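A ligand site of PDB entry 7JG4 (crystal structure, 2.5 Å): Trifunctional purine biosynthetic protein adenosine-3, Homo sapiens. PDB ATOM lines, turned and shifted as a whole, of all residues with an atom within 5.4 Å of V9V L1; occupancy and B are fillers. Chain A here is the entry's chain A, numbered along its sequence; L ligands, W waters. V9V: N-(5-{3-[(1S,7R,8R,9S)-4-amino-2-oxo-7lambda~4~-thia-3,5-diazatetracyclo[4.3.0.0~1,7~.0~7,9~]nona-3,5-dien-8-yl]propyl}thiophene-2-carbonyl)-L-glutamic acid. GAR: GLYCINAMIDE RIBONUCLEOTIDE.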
ATOM      1  N   LYS A  38      23.416 -34.231  19.680  1.00  0.00           N
ATOM      2  CA  LYS A  38      23.472 -35.582  19.132  1.00  0.00           C
ATOM      3  C   LYS A  38      24.069 -36.512  20.182  1.00  0.00           C
ATOM      4  O   LYS A  38      25.083 -36.171  20.816  1.00  0.00           O
ATOM      5  CB  LYS A  38      24.273 -35.641  17.821  1.00  0.00           C
ATOM      6  CG  LYS A  38      23.697 -34.762  16.681  1.00  0.00           C
ATOM      7  CD  LYS A  38      24.598 -34.754  15.421  1.00  0.00           C
ATOM      8  CE  LYS A  38      24.103 -33.766  14.342  1.00  0.00           C
ATOM      9  NZ  LYS A  38      22.728 -34.079  13.830  1.00  0.00           N
ATOM     10  N   HIS A  59      17.439 -31.894  19.126  1.00  0.00           N
ATOM     11  CA  HIS A  59      16.563 -30.925  18.440  1.00  0.00           C
ATOM     12  C   HIS A  59      15.398 -31.580  17.730  1.00  0.00           C
ATOM     13  O   HIS A  59      14.644 -30.865  17.045  1.00  0.00           O
ATOM     14  CB  HIS A  59      17.385 -30.077  17.459  1.00  0.00           C
ATOM     15  CG  HIS A  59      17.963 -30.859  16.307  1.00  0.00           C
ATOM     16  ND1 HIS A  59      18.503 -32.121  16.457  1.00  0.00           N
ATOM     17  CD2 HIS A  59      18.078 -30.547  14.994  1.00  0.00           C
ATOM     18  CE1 HIS A  59      18.935 -32.548  15.279  1.00  0.00           C
ATOM     19  NE2 HIS A  59      18.687 -31.613  14.380  1.00  0.00           N
ATOM     20  N   ARG A  65      12.385 -24.323  16.517  1.00  0.00           N
ATOM     21  CA  ARG A  65      13.748 -24.044  16.959  1.00  0.00           C
ATOM     22  C   ARG A  65      13.775 -23.344  18.304  1.00  0.00           C
ATOM     23  O   ARG A  65      14.588 -23.690  19.180  1.00  0.00           O
ATOM     24  CB  ARG A  65      14.470 -23.200  15.919  1.00  0.00           C
ATOM     25  CG  ARG A  65      15.464 -23.973  15.092  1.00  0.00           C
ATOM     26  CD  ARG A  65      16.253 -23.055  14.178  1.00  0.00           C
ATOM     27  NE  ARG A  65      17.173 -23.805  13.312  1.00  0.00           N
ATOM     28  CZ  ARG A  65      17.065 -23.872  11.994  1.00  0.00           C
ATOM     29  NH1 ARG A  65      16.096 -23.216  11.361  1.00  0.00           N
ATOM     30  NH2 ARG A  65      17.943 -24.577  11.295  1.00  0.00           N
ATOM     31  N   LEU A  86      30.384 -22.395  20.823  1.00  0.00           N
ATOM     32  CA  LEU A  86      29.939 -23.318  19.787  1.00  0.00           C
ATOM     33  C   LEU A  86      31.164 -23.987  19.176  1.00  0.00           C
ATOM     34  O   LEU A  86      31.949 -23.332  18.457  1.00  0.00           O
ATOM     35  CB  LEU A  86      29.127 -22.565  18.737  1.00  0.00           C
ATOM     36  CG  LEU A  86      27.968 -21.726  19.266  1.00  0.00           C
ATOM     37  CD1 LEU A  86      27.184 -21.138  18.117  1.00  0.00           C
ATOM     38  CD2 LEU A  86      27.056 -22.517  20.227  1.00  0.00           C
ATOM     39  N   PHE A  89      29.139 -27.265  16.811  1.00  0.00           N
ATOM     40  CA  PHE A  89      27.696 -27.319  16.973  1.00  0.00           C
ATOM     41  C   PHE A  89      27.060 -26.932  15.640  1.00  0.00           C
ATOM     42  O   PHE A  89      27.348 -25.852  15.106  1.00  0.00           O
ATOM     43  CB  PHE A  89      27.284 -26.369  18.094  1.00  0.00           C
ATOM     44  CG  PHE A  89      25.847 -26.428  18.426  1.00  0.00           C
ATOM     45  CD1 PHE A  89      25.353 -27.464  19.213  1.00  0.00           C
ATOM     46  CD2 PHE A  89      24.985 -25.453  17.973  1.00  0.00           C
ATOM     47  CE1 PHE A  89      24.007 -27.516  19.541  1.00  0.00           C
ATOM     48  CE2 PHE A  89      23.637 -25.499  18.294  1.00  0.00           C
ATOM     49  CZ  PHE A  89      23.153 -26.533  19.081  1.00  0.00           C
ATOM     50  N   MET A  90      26.229 -27.805  15.099  1.00  0.00           N
ATOM     51  CA  MET A  90      25.798 -27.675  13.713  1.00  0.00           C
ATOM     52  C   MET A  90      24.324 -27.304  13.586  1.00  0.00           C
ATOM     53  O   MET A  90      23.677 -27.598  12.573  1.00  0.00           O
ATOM     54  CB  MET A  90      26.081 -28.959  12.928  1.00  0.00           C
ATOM     55  CG  MET A  90      27.574 -29.288  12.820  1.00  0.00           C
ATOM     56  SD  MET A  90      28.622 -27.936  12.185  1.00  0.00           S
ATOM     57  CE  MET A  90      27.770 -27.500  10.652  1.00  0.00           C
ATOM     58  N   ARG A  91      23.779 -26.645  14.609  1.00  0.00           N
ATOM     59  CA  ARG A  91      22.437 -26.098  14.571  1.00  0.00           C
ATOM     60  C   ARG A  91      22.504 -24.582  14.443  1.00  0.00           C
ATOM     61  O   ARG A  91      23.433 -23.945  14.962  1.00  0.00           O
ATOM     62  CB  ARG A  91      21.652 -26.454  15.829  1.00  0.00           C
ATOM     63  CG  ARG A  91      21.515 -27.932  16.080  1.00  0.00           C
ATOM     64  CD  ARG A  91      20.870 -28.594  14.885  1.00  0.00           C
ATOM     65  NE  ARG A  91      19.837 -27.737  14.319  1.00  0.00           N
ATOM     66  CZ  ARG A  91      19.133 -28.044  13.233  1.00  0.00           C
ATOM     67  NH1 ARG A  91      19.342 -29.202  12.611  1.00  0.00           N
ATOM     68  NH2 ARG A  91      18.212 -27.207  12.785  1.00  0.00           N
ATOM     69  N   ILE A  92      21.540 -24.014  13.772  1.00  0.00           N
ATOM     70  CA  ILE A  92      21.442 -22.562  13.727  1.00  0.00           C
ATOM     71  C   ILE A  92      20.562 -22.107  14.875  1.00  0.00           C
ATOM     72  O   ILE A  92      19.502 -22.683  15.143  1.00  0.00           O
ATOM     73  CB  ILE A  92      20.900 -22.061  12.377  1.00  0.00           C
ATOM     74  CG1 ILE A  92      21.884 -22.404  11.277  1.00  0.00           C
ATOM     75  CG2 ILE A  92      20.693 -20.571  12.433  1.00  0.00           C
ATOM     76  CD1 ILE A  92      21.435 -21.975   9.905  1.00  0.00           C
ATOM     77  N   LEU A  93      21.007 -21.064  15.574  1.00  0.00           N
ATOM     78  CA  LEU A  93      20.322 -20.634  16.772  1.00  0.00           C
ATOM     79  C   LEU A  93      19.290 -19.566  16.424  1.00  0.00           C
ATOM     80  O   LEU A  93      19.471 -18.773  15.496  1.00  0.00           O
ATOM     81  CB  LEU A  93      21.338 -20.116  17.795  1.00  0.00           C
ATOM     82  CG  LEU A  93      22.264 -21.285  18.172  1.00  0.00           C
ATOM     83  CD1 LEU A  93      23.565 -20.841  18.825  1.00  0.00           C
ATOM     84  CD2 LEU A  93      21.523 -22.247  19.069  1.00  0.00           C
ATOM     85  N   VAL A  98      20.166 -15.842  20.177  1.00  0.00           N
ATOM     86  CA  VAL A  98      21.379 -15.125  19.802  1.00  0.00           C
ATOM     87  C   VAL A  98      21.376 -13.728  20.399  1.00  0.00           C
ATOM     88  O   VAL A  98      22.411 -13.241  20.864  1.00  0.00           O
ATOM     89  CB  VAL A  98      21.521 -15.077  18.261  1.00  0.00           C
ATOM     90  CG1 VAL A  98      22.799 -14.322  17.858  1.00  0.00           C
ATOM     91  CG2 VAL A  98      21.536 -16.486  17.678  1.00  0.00           C
ATOM     92  N   ASN A 107      31.853 -18.664  18.229  1.00  0.00           N
ATOM     93  CA  ASN A 107      31.766 -19.756  17.282  1.00  0.00           C
ATOM     94  C   ASN A 107      33.081 -19.880  16.529  1.00  0.00           C
ATOM     95  O   ASN A 107      33.719 -18.877  16.223  1.00  0.00           O
ATOM     96  CB  ASN A 107      30.634 -19.545  16.281  1.00  0.00           C
ATOM     97  CG  ASN A 107      30.586 -20.614  15.229  1.00  0.00           C
ATOM     98  OD1 ASN A 107      30.369 -21.787  15.535  1.00  0.00           O
ATOM     99  ND2 ASN A 107      30.811 -20.239  13.973  1.00  0.00           N
ATOM    100  N   HIS A 109      34.677 -21.289  13.030  1.00  0.00           N
ATOM    101  CA  HIS A 109      34.314 -21.592  11.651  1.00  0.00           C
ATOM    102  C   HIS A 109      35.597 -21.830  10.867  1.00  0.00           C
ATOM    103  O   HIS A 109      36.551 -21.029  10.990  1.00  0.00           O
ATOM    104  CB  HIS A 109      33.502 -20.461  11.024  1.00  0.00           C
ATOM    105  CG  HIS A 109      33.098 -20.687   9.597  1.00  0.00           C
ATOM    106  ND1 HIS A 109      32.003 -21.456   9.249  1.00  0.00           N
ATOM    107  CD2 HIS A 109      33.622 -20.231   8.433  1.00  0.00           C
ATOM    108  CE1 HIS A 109      31.884 -21.460   7.935  1.00  0.00           C
ATOM    109  NE2 HIS A 109      32.844 -20.725   7.417  1.00  0.00           N
ATOM    110  N   GLY A 118      28.869 -20.896   5.853  1.00  0.00           N
ATOM    111  CA  GLY A 118      28.079 -22.092   5.760  1.00  0.00           C
ATOM    112  C   GLY A 118      28.836 -23.352   6.143  1.00  0.00           C
ATOM    113  O   GLY A 118      29.955 -23.337   6.660  1.00  0.00           O
ATOM    114  N   SER A 119      28.190 -24.470   5.860  1.00  0.00           N
ATOM    115  CA  SER A 119      28.525 -25.733   6.520  1.00  0.00           C
ATOM    116  C   SER A 119      29.621 -26.533   5.832  1.00  0.00           C
ATOM    117  O   SER A 119      30.088 -27.528   6.408  1.00  0.00           O
ATOM    118  CB  SER A 119      27.260 -26.586   6.631  1.00  0.00           C
ATOM    119  OG  SER A 119      26.542 -26.528   5.415  1.00  0.00           O
ATOM    120  N   HIS A 138      34.620 -15.969  16.075  1.00  0.00           N
ATOM    121  CA  HIS A 138      33.848 -14.738  16.032  1.00  0.00           C
ATOM    122  C   HIS A 138      32.701 -14.812  17.033  1.00  0.00           C
ATOM    123  O   HIS A 138      32.266 -15.900  17.442  1.00  0.00           O
ATOM    124  CB  HIS A 138      33.276 -14.487  14.637  1.00  0.00           C
ATOM    125  CG  HIS A 138      32.263 -15.505  14.217  1.00  0.00           C
ATOM    126  ND1 HIS A 138      30.906 -15.252  14.240  1.00  0.00           N
ATOM    127  CD2 HIS A 138      32.404 -16.773  13.774  1.00  0.00           C
ATOM    128  CE1 HIS A 138      30.256 -16.328  13.820  1.00  0.00           C
ATOM    129  NE2 HIS A 138      31.141 -17.263  13.535  1.00  0.00           N
ATOM    130  N   VAL A 140      28.883 -14.756  17.872  1.00  0.00           N
ATOM    131  CA  VAL A 140      27.709 -15.150  17.101  1.00  0.00           C
ATOM    132  C   VAL A 140      26.755 -13.971  17.019  1.00  0.00           C
ATOM    133  O   VAL A 140      26.292 -13.449  18.044  1.00  0.00           O
ATOM    134  CB  VAL A 140      27.050 -16.392  17.708  1.00  0.00           C
ATOM    135  CG1 VAL A 140      25.792 -16.770  16.948  1.00  0.00           C
ATOM    136  CG2 VAL A 140      28.044 -17.554  17.719  1.00  0.00           C
ATOM    137  N   ALA A 141      26.490 -13.519  15.809  1.00  0.00           N
ATOM    138  CA  ALA A 141      25.457 -12.518  15.562  1.00  0.00           C
ATOM    139  C   ALA A 141      24.267 -13.217  14.910  1.00  0.00           C
ATOM    140  O   ALA A 141      24.292 -14.422  14.673  1.00  0.00           O
ATOM    141  CB  ALA A 141      25.996 -11.372  14.694  1.00  0.00           C
ATOM    142  N   GLU A 142      23.220 -12.443  14.610  1.00  0.00           N
ATOM    143  CA  GLU A 142      22.015 -13.060  14.074  1.00  0.00           C
ATOM    144  C   GLU A 142      22.250 -13.621  12.676  1.00  0.00           C
ATOM    145  O   GLU A 142      21.849 -14.752  12.379  1.00  0.00           O
ATOM    146  CB  GLU A 142      20.856 -12.074  14.086  1.00  0.00           C
ATOM    147  CG  GLU A 142      19.888 -12.349  15.236  1.00  0.00           C
ATOM    148  CD  GLU A 142      18.547 -11.658  15.071  1.00  0.00           C
ATOM    149  OE1 GLU A 142      17.920 -11.815  14.003  1.00  0.00           O
ATOM    150  OE2 GLU A 142      18.118 -10.948  16.018  1.00  0.00           O
ATOM    151  N   ASP A 143      22.901 -12.860  11.799  1.00  0.00           N
ATOM    152  CA  ASP A 143      23.252 -13.398  10.488  1.00  0.00           C
ATOM    153  C   ASP A 143      24.501 -14.272  10.595  1.00  0.00           C
ATOM    154  O   ASP A 143      25.515 -13.855  11.161  1.00  0.00           O
ATOM    155  CB  ASP A 143      23.442 -12.264   9.475  1.00  0.00           C
ATOM    156  CG  ASP A 143      24.791 -11.595   9.595  1.00  0.00           C
ATOM    157  OD1 ASP A 143      25.279 -11.405  10.735  1.00  0.00           O
ATOM    158  OD2 ASP A 143      25.361 -11.255   8.536  1.00  0.00           O
ATOM    159  N   VAL A 144      24.414 -15.487  10.050  1.00  0.00           N
ATOM    160  CA  VAL A 144      25.393 -16.537  10.354  1.00  0.00           C
ATOM    161  C   VAL A 144      26.774 -16.159   9.829  1.00  0.00           C
ATOM    162  O   VAL A 144      26.923 -15.586   8.746  1.00  0.00           O
ATOM    163  CB  VAL A 144      24.911 -17.880   9.781  1.00  0.00           C
ATOM    164  CG1 VAL A 144      25.943 -18.996  10.018  1.00  0.00           C
ATOM    165  CG2 VAL A 144      23.569 -18.263  10.378  1.00  0.00           C
ATOM    166  N   ASP A 145      27.799 -16.489  10.626  1.00  0.00           N
ATOM    167  CA  ASP A 145      29.202 -16.273  10.251  1.00  0.00           C
ATOM    168  C   ASP A 145      29.432 -14.833   9.778  1.00  0.00           C
ATOM    169  O   ASP A 145      30.193 -14.573   8.842  1.00  0.00           O
ATOM    170  CB  ASP A 145      29.662 -17.283   9.205  1.00  0.00           C
ATOM    171  CG  ASP A 145      29.271 -18.710   9.559  1.00  0.00           C
ATOM    172  OD1 ASP A 145      29.170 -19.026  10.773  1.00  0.00           O
ATOM    173  OD2 ASP A 145      29.058 -19.520   8.625  1.00  0.00           O
ATOM    174  N   ALA A 146      28.749 -13.891  10.437  1.00  0.00           N
ATOM    175  CA  ALA A 146      28.956 -12.473  10.191  1.00  0.00           C
ATOM    176  C   ALA A 146      28.876 -11.656  11.477  1.00  0.00           C
ATOM    177  O   ALA A 146      28.596 -10.456  11.430  1.00  0.00           O
ATOM    178  CB  ALA A 146      27.954 -11.928   9.165  1.00  0.00           C
HETATM  179  C8  V9V L   1      25.840 -19.228  13.983  1.00  0.00           C
HETATM  180  C6  V9V L   1      26.587 -21.320  14.374  1.00  0.00           C
HETATM  181  N1  V9V L   1      23.495 -19.153  14.557  1.00  0.00           N
HETATM  182  C2  V9V L   1      23.538 -17.832  14.189  1.00  0.00           C
HETATM  183  N3  V9V L   1      24.584 -17.144  13.739  1.00  0.00           N
HETATM  184  C4  V9V L   1      25.747 -17.813  13.621  1.00  0.00           C
HETATM  185  C7  V9V L   1      26.988 -20.139  13.932  1.00  0.00           C
HETATM  186  C13 V9V L   1      25.065 -23.955   9.314  1.00  0.00           C
HETATM  187  C14 V9V L   1      25.992 -22.991   9.046  1.00  0.00           C
HETATM  188  C15 V9V L   1      26.899 -22.864  10.068  1.00  0.00           C
HETATM  189  C16 V9V L   1      26.711 -23.702  11.119  1.00  0.00           C
HETATM  190  C17 V9V L   1      23.927 -24.451   8.542  1.00  0.00           C
HETATM  191  C20 V9V L   1      22.018 -26.122   8.801  1.00  0.00           C
HETATM  192  C21 V9V L   1      22.386 -27.613   8.779  1.00  0.00           C
HETATM  193  C22 V9V L   1      21.864 -28.351  10.027  1.00  0.00           C
HETATM  194  C23 V9V L   1      22.690 -29.540  10.466  1.00  0.00           C
HETATM  195  C26 V9V L   1      20.880 -25.873   9.781  1.00  0.00           C
HETATM  196  C29 V9V L   1      27.464 -22.519  14.448  1.00  0.00           C
HETATM  197  C30 V9V L   1      27.983 -22.565  13.007  1.00  0.00           C
HETATM  198  C31 V9V L   1      27.494 -23.854  12.389  1.00  0.00           C
HETATM  199  C9  V9V L   1      24.672 -19.855  14.448  1.00  0.00           C
HETATM  200  N11 V9V L   1      22.374 -17.150  14.292  1.00  0.00           N
HETATM  201  N19 V9V L   1      23.206 -25.377   9.225  1.00  0.00           N
HETATM  202  O10 V9V L   1      26.748 -17.231  13.217  1.00  0.00           O
HETATM  203  O18 V9V L   1      23.690 -24.056   7.412  1.00  0.00           O
HETATM  204  O24 V9V L   1      22.244 -30.308  11.286  1.00  0.00           O
HETATM  205  O25 V9V L   1      23.910 -29.746   9.947  1.00  0.00           O
HETATM  206  O27 V9V L   1      21.046 -25.890  10.977  1.00  0.00           O
HETATM  207  O28 V9V L   1      19.638 -25.626   9.313  1.00  0.00           O
HETATM  208  S12 V9V L   1      25.366 -24.692  10.871  1.00  0.00           S
HETATM  209  S5  V9V L   1      24.913 -21.165  14.739  1.00  0.00           S
HETATM  210  C1  GAR L   2      35.466 -27.887  13.180  1.00  0.00           C
HETATM  211  O6  GAR L   2      36.406 -28.097  12.150  1.00  0.00           O
HETATM  212  C2  GAR L   2      34.706 -26.570  12.943  1.00  0.00           C
HETATM  213  O8  GAR L   2      35.419 -25.590  12.229  1.00  0.00           O
HETATM  214  C3  GAR L   2      33.453 -27.041  12.180  1.00  0.00           C
HETATM  215  O4  GAR L   2      33.205 -28.373  12.697  1.00  0.00           O
HETATM  216  C5  GAR L   2      34.418 -29.006  13.160  1.00  0.00           C
HETATM  217  C10 GAR L   2      34.202 -29.648  14.512  1.00  0.00           C
HETATM  218  O12 GAR L   2      35.338 -30.424  14.908  1.00  0.00           O
HETATM  219  N19 GAR L   2      32.328 -26.164  12.332  1.00  0.00           N
HETATM  220  C21 GAR L   2      31.725 -25.645  11.250  1.00  0.00           C
HETATM  221  O22 GAR L   2      31.962 -25.994  10.083  1.00  0.00           O
HETATM  222  C23 GAR L   2      30.699 -24.581  11.546  1.00  0.00           C
HETATM  223  N24 GAR L   2      30.081 -24.070  10.335  1.00  0.00           N
HETATM  224  P15 GAR L   2      35.417 -30.969  16.422  1.00  0.00           P
HETATM  225  O16 GAR L   2      35.750 -29.751  17.264  1.00  0.00           O
HETATM  226  O17 GAR L   2      36.497 -32.020  16.374  1.00  0.00           O
HETATM  227  O18 GAR L   2      34.032 -31.532  16.685  1.00  0.00           O
HETATM  228  O   HOH W   1      29.382 -24.417  15.795  1.00  0.00           O
HETATM  229  O   HOH W   2      27.200 -14.726  13.313  1.00  0.00           O
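O of His 138 sits at hydrogen-bond distance from N of Asn 107 (2.9 Å).
The backbone carbonyl oxygen (O) of Ile 92 is in hydrogen-bond range of the guanidinium group (NE) of Arg 65.
The backbone NH of Gly 118 lies within hydrogen-bond range of the side-chain carboxylate of Asp 145, 3.1 Å away.
NE2 of His 59 sits close to NH1 of Arg 91, 3.1 Å away.
Water W1 bridges O of Phe 89 (2.6 Å) and OD1 of Asn 107 (2.8 Å).
The backbone carbonyl oxygen (O) of Met 90 lies close to an oxygen (O24) of V9V L1, 3.3 Å away.
Merely in contact with V9V L1: Leu 86 (3.8 Å), Phe 89 (3.4 Å), Val 98 (3.6 Å), Asn 107 (3.2 Å), Gly 118 (3.995 Å), His 138 (3.7 Å), Val 140 (3.4 Å) and Val 144 (3.2 Å).
Hydrophobic or aromatic side chains that line V9V L1: Leu 86, Met 90, Ile 92, Val 98, His 138, Val 140 and Val 144.
Within 4 Å of V9V L1: Arg 65, Leu 86, Phe 89, Met 90, Arg 91, Ile 92, Leu 93, Val 98, Asn 107, Gly 118, His 138, Val 140, Ala 141, Glu 142, Val 144 and Asp 145.
The nearest printed residue that does not touch V9V L1 is Asp 143 (4.1 Å).
N of Ile 92 sits at hydrogen-bond distance from O27 of V9V L1, 3.4 Å away.
The guanidinium group of Arg 65 is in salt-bridge range of an oxygen (O28) of V9V L1 (2.8 Å).
An oxygen (O24) of V9V L1 is in salt-bridge range of the guanidinium group (NH1) of Arg 91 (3.4 Å).
ND1 of His 109 lies within hydrogen-bond range of N24 of GAR L2.
A nitrogen (N11) of V9V L1 lies within hydrogen-bond range of the backbone carbonyl oxygen (O) of Glu 142 (3.1 Å).
The backbone NH (N) of Asp 145 is in hydrogen-bond range of an oxygen (O10) of V9V L1 (2.9 Å).
The backbone NH (N) of Leu 93 lies within hydrogen-bond range of a nitrogen (N1) of V9V L1 (3.3 Å).
The backbone carbonyl oxygen (O) of Ala 141 sits at hydrogen-bond distance from a nitrogen (N3) of V9V L1 (2.9 Å).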
